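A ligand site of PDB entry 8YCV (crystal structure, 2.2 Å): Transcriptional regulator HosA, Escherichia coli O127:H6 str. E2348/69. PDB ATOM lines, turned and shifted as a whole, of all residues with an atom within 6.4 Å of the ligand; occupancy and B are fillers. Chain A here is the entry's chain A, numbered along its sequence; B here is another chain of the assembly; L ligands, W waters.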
ATOM      1  N   LEU A   3     -23.350 -22.055 -24.946  1.00  0.00           N
ATOM      2  CA  LEU A   3     -23.185 -23.493 -25.095  1.00  0.00           C
ATOM      3  C   LEU A   3     -24.191 -24.279 -24.258  1.00  0.00           C
ATOM      4  O   LEU A   3     -24.565 -25.391 -24.630  1.00  0.00           O
ATOM      5  CB  LEU A   3     -21.761 -23.890 -24.717  1.00  0.00           C
ATOM      6  CG  LEU A   3     -20.731 -23.763 -25.852  1.00  0.00           C
ATOM      7  CD1 LEU A   3     -19.337 -23.625 -25.281  1.00  0.00           C
ATOM      8  CD2 LEU A   3     -20.820 -24.977 -26.765  1.00  0.00           C
ATOM      9  N   LYS A   6     -27.110 -25.714 -26.159  1.00  0.00           N
ATOM     10  CA  LYS A   6     -26.907 -26.764 -27.153  1.00  0.00           C
ATOM     11  C   LYS A   6     -27.179 -28.116 -26.486  1.00  0.00           C
ATOM     12  O   LYS A   6     -26.521 -28.476 -25.507  1.00  0.00           O
ATOM     13  CB  LYS A   6     -25.497 -26.707 -27.721  1.00  0.00           C
ATOM     14  CG  LYS A   6     -25.245 -25.499 -28.625  1.00  0.00           C
ATOM     15  CD  LYS A   6     -25.965 -25.640 -29.967  1.00  0.00           C
ATOM     16  CE  LYS A   6     -25.766 -24.395 -30.836  1.00  0.00           C
ATOM     17  NZ  LYS A   6     -26.560 -24.466 -32.098  1.00  0.00           N
ATOM     18  N   ALA A   7     -28.143 -28.858 -27.041  1.00  0.00           N
ATOM     19  CA  ALA A   7     -28.528 -30.122 -26.437  1.00  0.00           C
ATOM     20  C   ALA A   7     -27.340 -31.086 -26.324  1.00  0.00           C
ATOM     21  O   ALA A   7     -27.192 -31.767 -25.310  1.00  0.00           O
ATOM     22  CB  ALA A   7     -29.652 -30.775 -27.246  1.00  0.00           C
ATOM     23  N   PHE A   8     -26.501 -31.145 -27.357  1.00  0.00           N
ATOM     24  CA  PHE A   8     -25.399 -32.101 -27.323  1.00  0.00           C
ATOM     25  C   PHE A   8     -24.235 -31.613 -26.478  1.00  0.00           C
ATOM     26  O   PHE A   8     -23.397 -32.427 -26.080  1.00  0.00           O
ATOM     27  CB  PHE A   8     -24.947 -32.436 -28.743  1.00  0.00           C
ATOM     28  CG  PHE A   8     -25.736 -33.543 -29.367  1.00  0.00           C
ATOM     29  CD1 PHE A   8     -25.465 -34.866 -29.057  1.00  0.00           C
ATOM     30  CD2 PHE A   8     -26.773 -33.273 -30.242  1.00  0.00           C
ATOM     31  CE1 PHE A   8     -26.196 -35.899 -29.608  1.00  0.00           C
ATOM     32  CE2 PHE A   8     -27.504 -34.295 -30.810  1.00  0.00           C
ATOM     33  CZ  PHE A   8     -27.222 -35.611 -30.495  1.00  0.00           C
ATOM     34  N   HIS A   9     -24.156 -30.320 -26.182  1.00  0.00           N
ATOM     35  CA  HIS A   9     -23.180 -29.873 -25.199  1.00  0.00           C
ATOM     36  C   HIS A   9     -23.599 -30.288 -23.791  1.00  0.00           C
ATOM     37  O   HIS A   9     -22.817 -30.907 -23.063  1.00  0.00           O
ATOM     38  CB  HIS A   9     -22.996 -28.356 -25.257  1.00  0.00           C
ATOM     39  CG  HIS A   9     -22.018 -27.839 -24.252  1.00  0.00           C
ATOM     40  ND1 HIS A   9     -20.659 -27.946 -24.426  1.00  0.00           N
ATOM     41  CD2 HIS A   9     -22.208 -27.242 -23.053  1.00  0.00           C
ATOM     42  CE1 HIS A   9     -20.039 -27.411 -23.377  1.00  0.00           C
ATOM     43  NE2 HIS A   9     -20.961 -26.981 -22.534  1.00  0.00           N
ATOM     44  N   GLN A  10     -24.828 -29.956 -23.408  1.00  0.00           N
ATOM     45  CA  GLN A  10     -25.347 -30.428 -22.123  1.00  0.00           C
ATOM     46  C   GLN A  10     -25.262 -31.935 -22.030  1.00  0.00           C
ATOM     47  O   GLN A  10     -25.068 -32.482 -20.940  1.00  0.00           O
ATOM     48  CB  GLN A  10     -26.783 -29.957 -21.927  1.00  0.00           C
ATOM     49  CG  GLN A  10     -26.938 -28.455 -21.749  1.00  0.00           C
ATOM     50  CD  GLN A  10     -26.144 -27.921 -20.567  1.00  0.00           C
ATOM     51  OE1 GLN A  10     -25.129 -27.242 -20.745  1.00  0.00           O
ATOM     52  NE2 GLN A  10     -26.595 -28.222 -19.359  1.00  0.00           N
ATOM     53  N   ARG A  12     -22.842 -33.883 -23.322  1.00  0.00           N
ATOM     54  CA  ARG A  12     -21.477 -34.204 -22.931  1.00  0.00           C
ATOM     55  C   ARG A  12     -21.221 -33.832 -21.467  1.00  0.00           C
ATOM     56  O   ARG A  12     -20.462 -34.516 -20.782  1.00  0.00           O
ATOM     57  CB  ARG A  12     -20.486 -33.490 -23.839  1.00  0.00           C
ATOM     58  CG  ARG A  12     -19.051 -33.970 -23.670  1.00  0.00           C
ATOM     59  CD  ARG A  12     -18.208 -33.610 -24.883  1.00  0.00           C
ATOM     60  NE  ARG A  12     -18.119 -32.172 -25.089  1.00  0.00           N
ATOM     61  CZ  ARG A  12     -17.183 -31.395 -24.560  1.00  0.00           C
ATOM     62  NH1 ARG A  12     -16.245 -31.887 -23.760  1.00  0.00           N
ATOM     63  NH2 ARG A  12     -17.191 -30.098 -24.836  1.00  0.00           N
ATOM     64  N   PHE B  15     -23.989 -40.661 -27.723  1.00  0.00           N
ATOM     65  CA  PHE B  15     -22.868 -39.738 -27.658  1.00  0.00           C
ATOM     66  C   PHE B  15     -21.760 -40.157 -28.612  1.00  0.00           C
ATOM     67  O   PHE B  15     -21.112 -39.309 -29.233  1.00  0.00           O
ATOM     68  CB  PHE B  15     -22.334 -39.665 -26.230  1.00  0.00           C
ATOM     69  CG  PHE B  15     -21.165 -38.750 -26.074  1.00  0.00           C
ATOM     70  CD1 PHE B  15     -21.360 -37.372 -26.048  1.00  0.00           C
ATOM     71  CD2 PHE B  15     -19.878 -39.238 -25.960  1.00  0.00           C
ATOM     72  CE1 PHE B  15     -20.282 -36.515 -25.907  1.00  0.00           C
ATOM     73  CE2 PHE B  15     -18.802 -38.389 -25.824  1.00  0.00           C
ATOM     74  CZ  PHE B  15     -19.008 -37.023 -25.794  1.00  0.00           C
ATOM     75  N   HIS B  18     -22.855 -39.493 -32.347  1.00  0.00           N
ATOM     76  CA  HIS B  18     -22.685 -38.071 -32.646  1.00  0.00           C
ATOM     77  C   HIS B  18     -21.218 -37.701 -32.711  1.00  0.00           C
ATOM     78  O   HIS B  18     -20.803 -36.922 -33.582  1.00  0.00           O
ATOM     79  CB  HIS B  18     -23.410 -37.240 -31.586  1.00  0.00           C
ATOM     80  CG  HIS B  18     -23.295 -35.760 -31.790  1.00  0.00           C
ATOM     81  ND1 HIS B  18     -22.246 -35.025 -31.286  1.00  0.00           N
ATOM     82  CD2 HIS B  18     -24.111 -34.879 -32.406  1.00  0.00           C
ATOM     83  CE1 HIS B  18     -22.413 -33.754 -31.605  1.00  0.00           C
ATOM     84  NE2 HIS B  18     -23.536 -33.634 -32.280  1.00  0.00           N
ATOM     85  N   TRP B  22     -19.224 -36.213 -35.956  1.00  0.00           N
ATOM     86  CA  TRP B  22     -18.392 -35.035 -35.787  1.00  0.00           C
ATOM     87  C   TRP B  22     -16.968 -35.285 -36.280  1.00  0.00           C
ATOM     88  O   TRP B  22     -16.375 -34.441 -36.952  1.00  0.00           O
ATOM     89  CB  TRP B  22     -18.363 -34.625 -34.312  1.00  0.00           C
ATOM     90  CG  TRP B  22     -17.910 -33.237 -34.070  1.00  0.00           C
ATOM     91  CD1 TRP B  22     -16.629 -32.776 -34.089  1.00  0.00           C
ATOM     92  CD2 TRP B  22     -18.736 -32.111 -33.763  1.00  0.00           C
ATOM     93  NE1 TRP B  22     -16.604 -31.422 -33.814  1.00  0.00           N
ATOM     94  CE2 TRP B  22     -17.894 -30.997 -33.611  1.00  0.00           C
ATOM     95  CE3 TRP B  22     -20.116 -31.937 -33.593  1.00  0.00           C
ATOM     96  CZ2 TRP B  22     -18.374 -29.724 -33.299  1.00  0.00           C
ATOM     97  CZ3 TRP B  22     -20.600 -30.681 -33.292  1.00  0.00           C
ATOM     98  CH2 TRP B  22     -19.731 -29.593 -33.145  1.00  0.00           C
ATOM     99  N   LYS B  31     -15.007 -31.878 -30.511  1.00  0.00           N
ATOM    100  CA  LYS B  31     -16.085 -31.171 -29.823  1.00  0.00           C
ATOM    101  C   LYS B  31     -15.555 -30.344 -28.656  1.00  0.00           C
ATOM    102  O   LYS B  31     -15.974 -29.175 -28.519  1.00  0.00           O
ATOM    103  CB  LYS B  31     -17.146 -32.178 -29.370  1.00  0.00           C
ATOM    104  CG  LYS B  31     -18.373 -32.226 -30.275  1.00  0.00           C
ATOM    105  CD  LYS B  31     -18.836 -33.652 -30.566  1.00  0.00           C
ATOM    106  CE  LYS B  31     -19.097 -34.437 -29.290  1.00  0.00           C
ATOM    107  NZ  LYS B  31     -20.073 -35.528 -29.512  1.00  0.00           N
ATOM    108  N   PRO B  32     -14.667 -30.861 -27.801  1.00  0.00           N
ATOM    109  CA  PRO B  32     -14.110 -29.989 -26.748  1.00  0.00           C
ATOM    110  C   PRO B  32     -13.327 -28.815 -27.298  1.00  0.00           C
ATOM    111  O   PRO B  32     -13.427 -27.703 -26.764  1.00  0.00           O
ATOM    112  CB  PRO B  32     -13.209 -30.949 -25.943  1.00  0.00           C
ATOM    113  CG  PRO B  32     -13.755 -32.322 -26.236  1.00  0.00           C
ATOM    114  CD  PRO B  32     -14.249 -32.266 -27.651  1.00  0.00           C
ATOM    115  N   TYR B  34     -13.890 -27.380 -30.225  1.00  0.00           N
ATOM    116  CA  TYR B  34     -14.915 -26.510 -30.780  1.00  0.00           C
ATOM    117  C   TYR B  34     -15.598 -25.690 -29.679  1.00  0.00           C
ATOM    118  O   TYR B  34     -15.746 -24.466 -29.801  1.00  0.00           O
ATOM    119  CB  TYR B  34     -15.932 -27.363 -31.539  1.00  0.00           C
ATOM    120  CG  TYR B  34     -17.164 -26.633 -32.020  1.00  0.00           C
ATOM    121  CD1 TYR B  34     -17.112 -25.783 -33.113  1.00  0.00           C
ATOM    122  CD2 TYR B  34     -18.387 -26.825 -31.395  1.00  0.00           C
ATOM    123  CE1 TYR B  34     -18.249 -25.123 -33.555  1.00  0.00           C
ATOM    124  CE2 TYR B  34     -19.526 -26.178 -31.834  1.00  0.00           C
ATOM    125  CZ  TYR B  34     -19.453 -25.328 -32.914  1.00  0.00           C
ATOM    126  OH  TYR B  34     -20.592 -24.681 -33.353  1.00  0.00           O
ATOM    127  N   ALA B  35     -16.000 -26.354 -28.600  1.00  0.00           N
ATOM    128  CA  ALA B  35     -16.682 -25.655 -27.519  1.00  0.00           C
ATOM    129  C   ALA B  35     -15.778 -24.608 -26.873  1.00  0.00           C
ATOM    130  O   ALA B  35     -16.211 -23.491 -26.579  1.00  0.00           O
ATOM    131  CB  ALA B  35     -17.175 -26.656 -26.470  1.00  0.00           C
ATOM    132  N   ARG B  38     -15.606 -21.565 -29.112  1.00  0.00           N
ATOM    133  CA  ARG B  38     -16.811 -20.744 -29.056  1.00  0.00           C
ATOM    134  C   ARG B  38     -16.894 -19.957 -27.755  1.00  0.00           C
ATOM    135  O   ARG B  38     -17.369 -18.819 -27.758  1.00  0.00           O
ATOM    136  CB  ARG B  38     -18.056 -21.612 -29.242  1.00  0.00           C
ATOM    137  CG  ARG B  38     -18.193 -22.176 -30.651  1.00  0.00           C
ATOM    138  CD  ARG B  38     -19.639 -22.426 -31.034  1.00  0.00           C
ATOM    139  NE  ARG B  38     -20.404 -21.190 -31.155  1.00  0.00           N
ATOM    140  CZ  ARG B  38     -21.621 -21.111 -31.667  1.00  0.00           C
ATOM    141  NH1 ARG B  38     -22.240 -22.173 -32.152  1.00  0.00           N
ATOM    142  NH2 ARG B  38     -22.235 -19.928 -31.714  1.00  0.00           N
ATOM    143  N   ALA B  54     -16.548 -25.041 -20.596  1.00  0.00           N
ATOM    144  CA  ALA B  54     -16.807 -25.328 -22.004  1.00  0.00           C
ATOM    145  C   ALA B  54     -16.137 -26.632 -22.418  1.00  0.00           C
ATOM    146  O   ALA B  54     -16.698 -27.390 -23.218  1.00  0.00           O
ATOM    147  CB  ALA B  54     -16.296 -24.172 -22.868  1.00  0.00           C
ATOM    148  N   VAL B  56     -15.499 -29.213 -20.501  1.00  0.00           N
ATOM    149  CA  VAL B  56     -15.960 -30.338 -19.700  1.00  0.00           C
ATOM    150  C   VAL B  56     -14.775 -31.265 -19.456  1.00  0.00           C
ATOM    151  O   VAL B  56     -14.858 -32.468 -19.704  1.00  0.00           O
ATOM    152  CB  VAL B  56     -17.126 -31.086 -20.369  1.00  0.00           C
ATOM    153  CG1 VAL B  56     -17.819 -31.980 -19.348  1.00  0.00           C
ATOM    154  CG2 VAL B  56     -18.119 -30.096 -20.988  1.00  0.00           C
ATOM    155  N   GLY B 106     -20.988 -28.232 -37.359  1.00  0.00           N
ATOM    156  CA  GLY B 106     -21.437 -28.824 -36.114  1.00  0.00           C
ATOM    157  C   GLY B 106     -22.944 -28.758 -35.945  1.00  0.00           C
ATOM    158  O   GLY B 106     -23.579 -29.734 -35.539  1.00  0.00           O
ATOM    159  N   ASP B 107     -23.532 -27.597 -36.245  1.00  0.00           N
ATOM    160  CA  ASP B 107     -24.979 -27.473 -36.180  1.00  0.00           C
ATOM    161  C   ASP B 107     -25.659 -28.568 -36.986  1.00  0.00           C
ATOM    162  O   ASP B 107     -26.613 -29.198 -36.513  1.00  0.00           O
ATOM    163  CB  ASP B 107     -25.407 -26.083 -36.675  1.00  0.00           C
ATOM    164  CG  ASP B 107     -25.135 -24.991 -35.649  1.00  0.00           C
ATOM    165  OD1 ASP B 107     -24.802 -25.316 -34.495  1.00  0.00           O
ATOM    166  OD2 ASP B 107     -25.256 -23.800 -36.007  1.00  0.00           O
ATOM    167  N   ASP B 110     -25.380 -31.927 -35.235  1.00  0.00           N
ATOM    168  CA  ASP B 110     -26.411 -31.938 -34.203  1.00  0.00           C
ATOM    169  C   ASP B 110     -27.787 -32.202 -34.808  1.00  0.00           C
ATOM    170  O   ASP B 110     -28.615 -32.884 -34.200  1.00  0.00           O
ATOM    171  CB  ASP B 110     -26.421 -30.603 -33.463  1.00  0.00           C
ATOM    172  CG  ASP B 110     -25.176 -30.390 -32.629  1.00  0.00           C
ATOM    173  OD1 ASP B 110     -24.359 -31.324 -32.524  1.00  0.00           O
ATOM    174  OD2 ASP B 110     -25.031 -29.282 -32.071  1.00  0.00           O
HETATM  175  C1  LIG L   1     -20.012 -30.151 -27.231  1.00  0.00           C
HETATM  176  O1  LIG L   1     -19.448 -29.360 -26.446  1.00  0.00           O
HETATM  177  O2  LIG L   1     -19.909 -31.404 -27.236  1.00  0.00           O
HETATM  178  C2  LIG L   1     -20.931 -29.536 -28.262  1.00  0.00           C
HETATM  179  C3  LIG L   1     -21.017 -28.150 -28.409  1.00  0.00           C
HETATM  180  C4  LIG L   1     -21.854 -27.571 -29.354  1.00  0.00           C
HETATM  181  C5  LIG L   1     -22.644 -28.376 -30.163  1.00  0.00           C
HETATM  182  C6  LIG L   1     -22.579 -29.761 -30.027  1.00  0.00           C
HETATM  183  C7  LIG L   1     -21.732 -30.328 -29.086  1.00  0.00           C
HETATM  184  O3  LIG L   1     -23.453 -27.769 -31.066  1.00  0.00           O
HETATM  185  O   HOH W   1     -21.248 -33.424 -27.280  1.00  0.00           O
HETATM  186  O   HOH W   2     -22.535 -26.220 -33.209  1.00  0.00           O
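The side-chain carboxylate (OD2) of Asp 110 of chain B is in hydrogen-bond range of an oxygen (O3) of the ligand (2.4 Å).
A ring nitrogen (ND1) of His 9 lies within hydrogen-bond range of an oxygen (O1) of the ligand (2.7 Å).
An oxygen (O1) of the ligand is in salt-bridge range of the guanidinium group of Arg 12 (2.9 Å).
NE2 of His 18 of chain B is in hydrogen-bond range of OD1 of Asp 110 of chain B (2.5 Å).
O of Ala 54 of chain B sits at hydrogen-bond distance from NH2 of Arg 12, at 3.2 Å.
The side-chain amino group (NZ) of Lys 6 lies within salt-bridge range of the side-chain carboxylate (OD1) of Asp 107 of chain B (3.1 Å).
NZ of Lys 31 of chain B sits at hydrogen-bond distance from ND1 of His 18 of chain B (2.8 Å).
The side-chain hydroxyl (OH) of Tyr 34 of chain B lies within hydrogen-bond range of the guanidinium group (NH1) of Arg 38 of chain B, 3.2 Å away.
Leu 3 touches the ligand (CD2 to C3, 3.6 Å).
Lys 6 touches the ligand.
Phe 8 touches the ligand.
Trp 22 of chain B touches the ligand (CZ3 to C6, 3.9 Å).
Lys 31 of chain B touches the ligand.
Tyr 34 of chain B touches the ligand.
Ala 35 of chain B touches the ligand.
Hydrophobic or aromatic side chains that line the ligand: Leu 3, Phe 8, His 9, Trp 22 of chain B, Tyr 34 of chain B and Ala 35 of chain B.
The nearest printed residue that does not touch the ligand is His 18 of chain B (4.3 Å).
Water W1 lies within hydrogen-bond range of an oxygen (O2) of the ligand (2.4 Å), the backbone carbonyl oxygen of Phe 8 (2.7 Å) and the side-chain amino group of Lys 31 of chain B (3.3 Å).
Water W2 lies within hydrogen-bond range of the side-chain hydroxyl (OH) of Tyr 34 of chain B (2.5 Å), the side-chain carboxylate (OD1) of Asp 107 of chain B (2.8 Å) and an oxygen (O3) of the ligand (2.8 Å).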
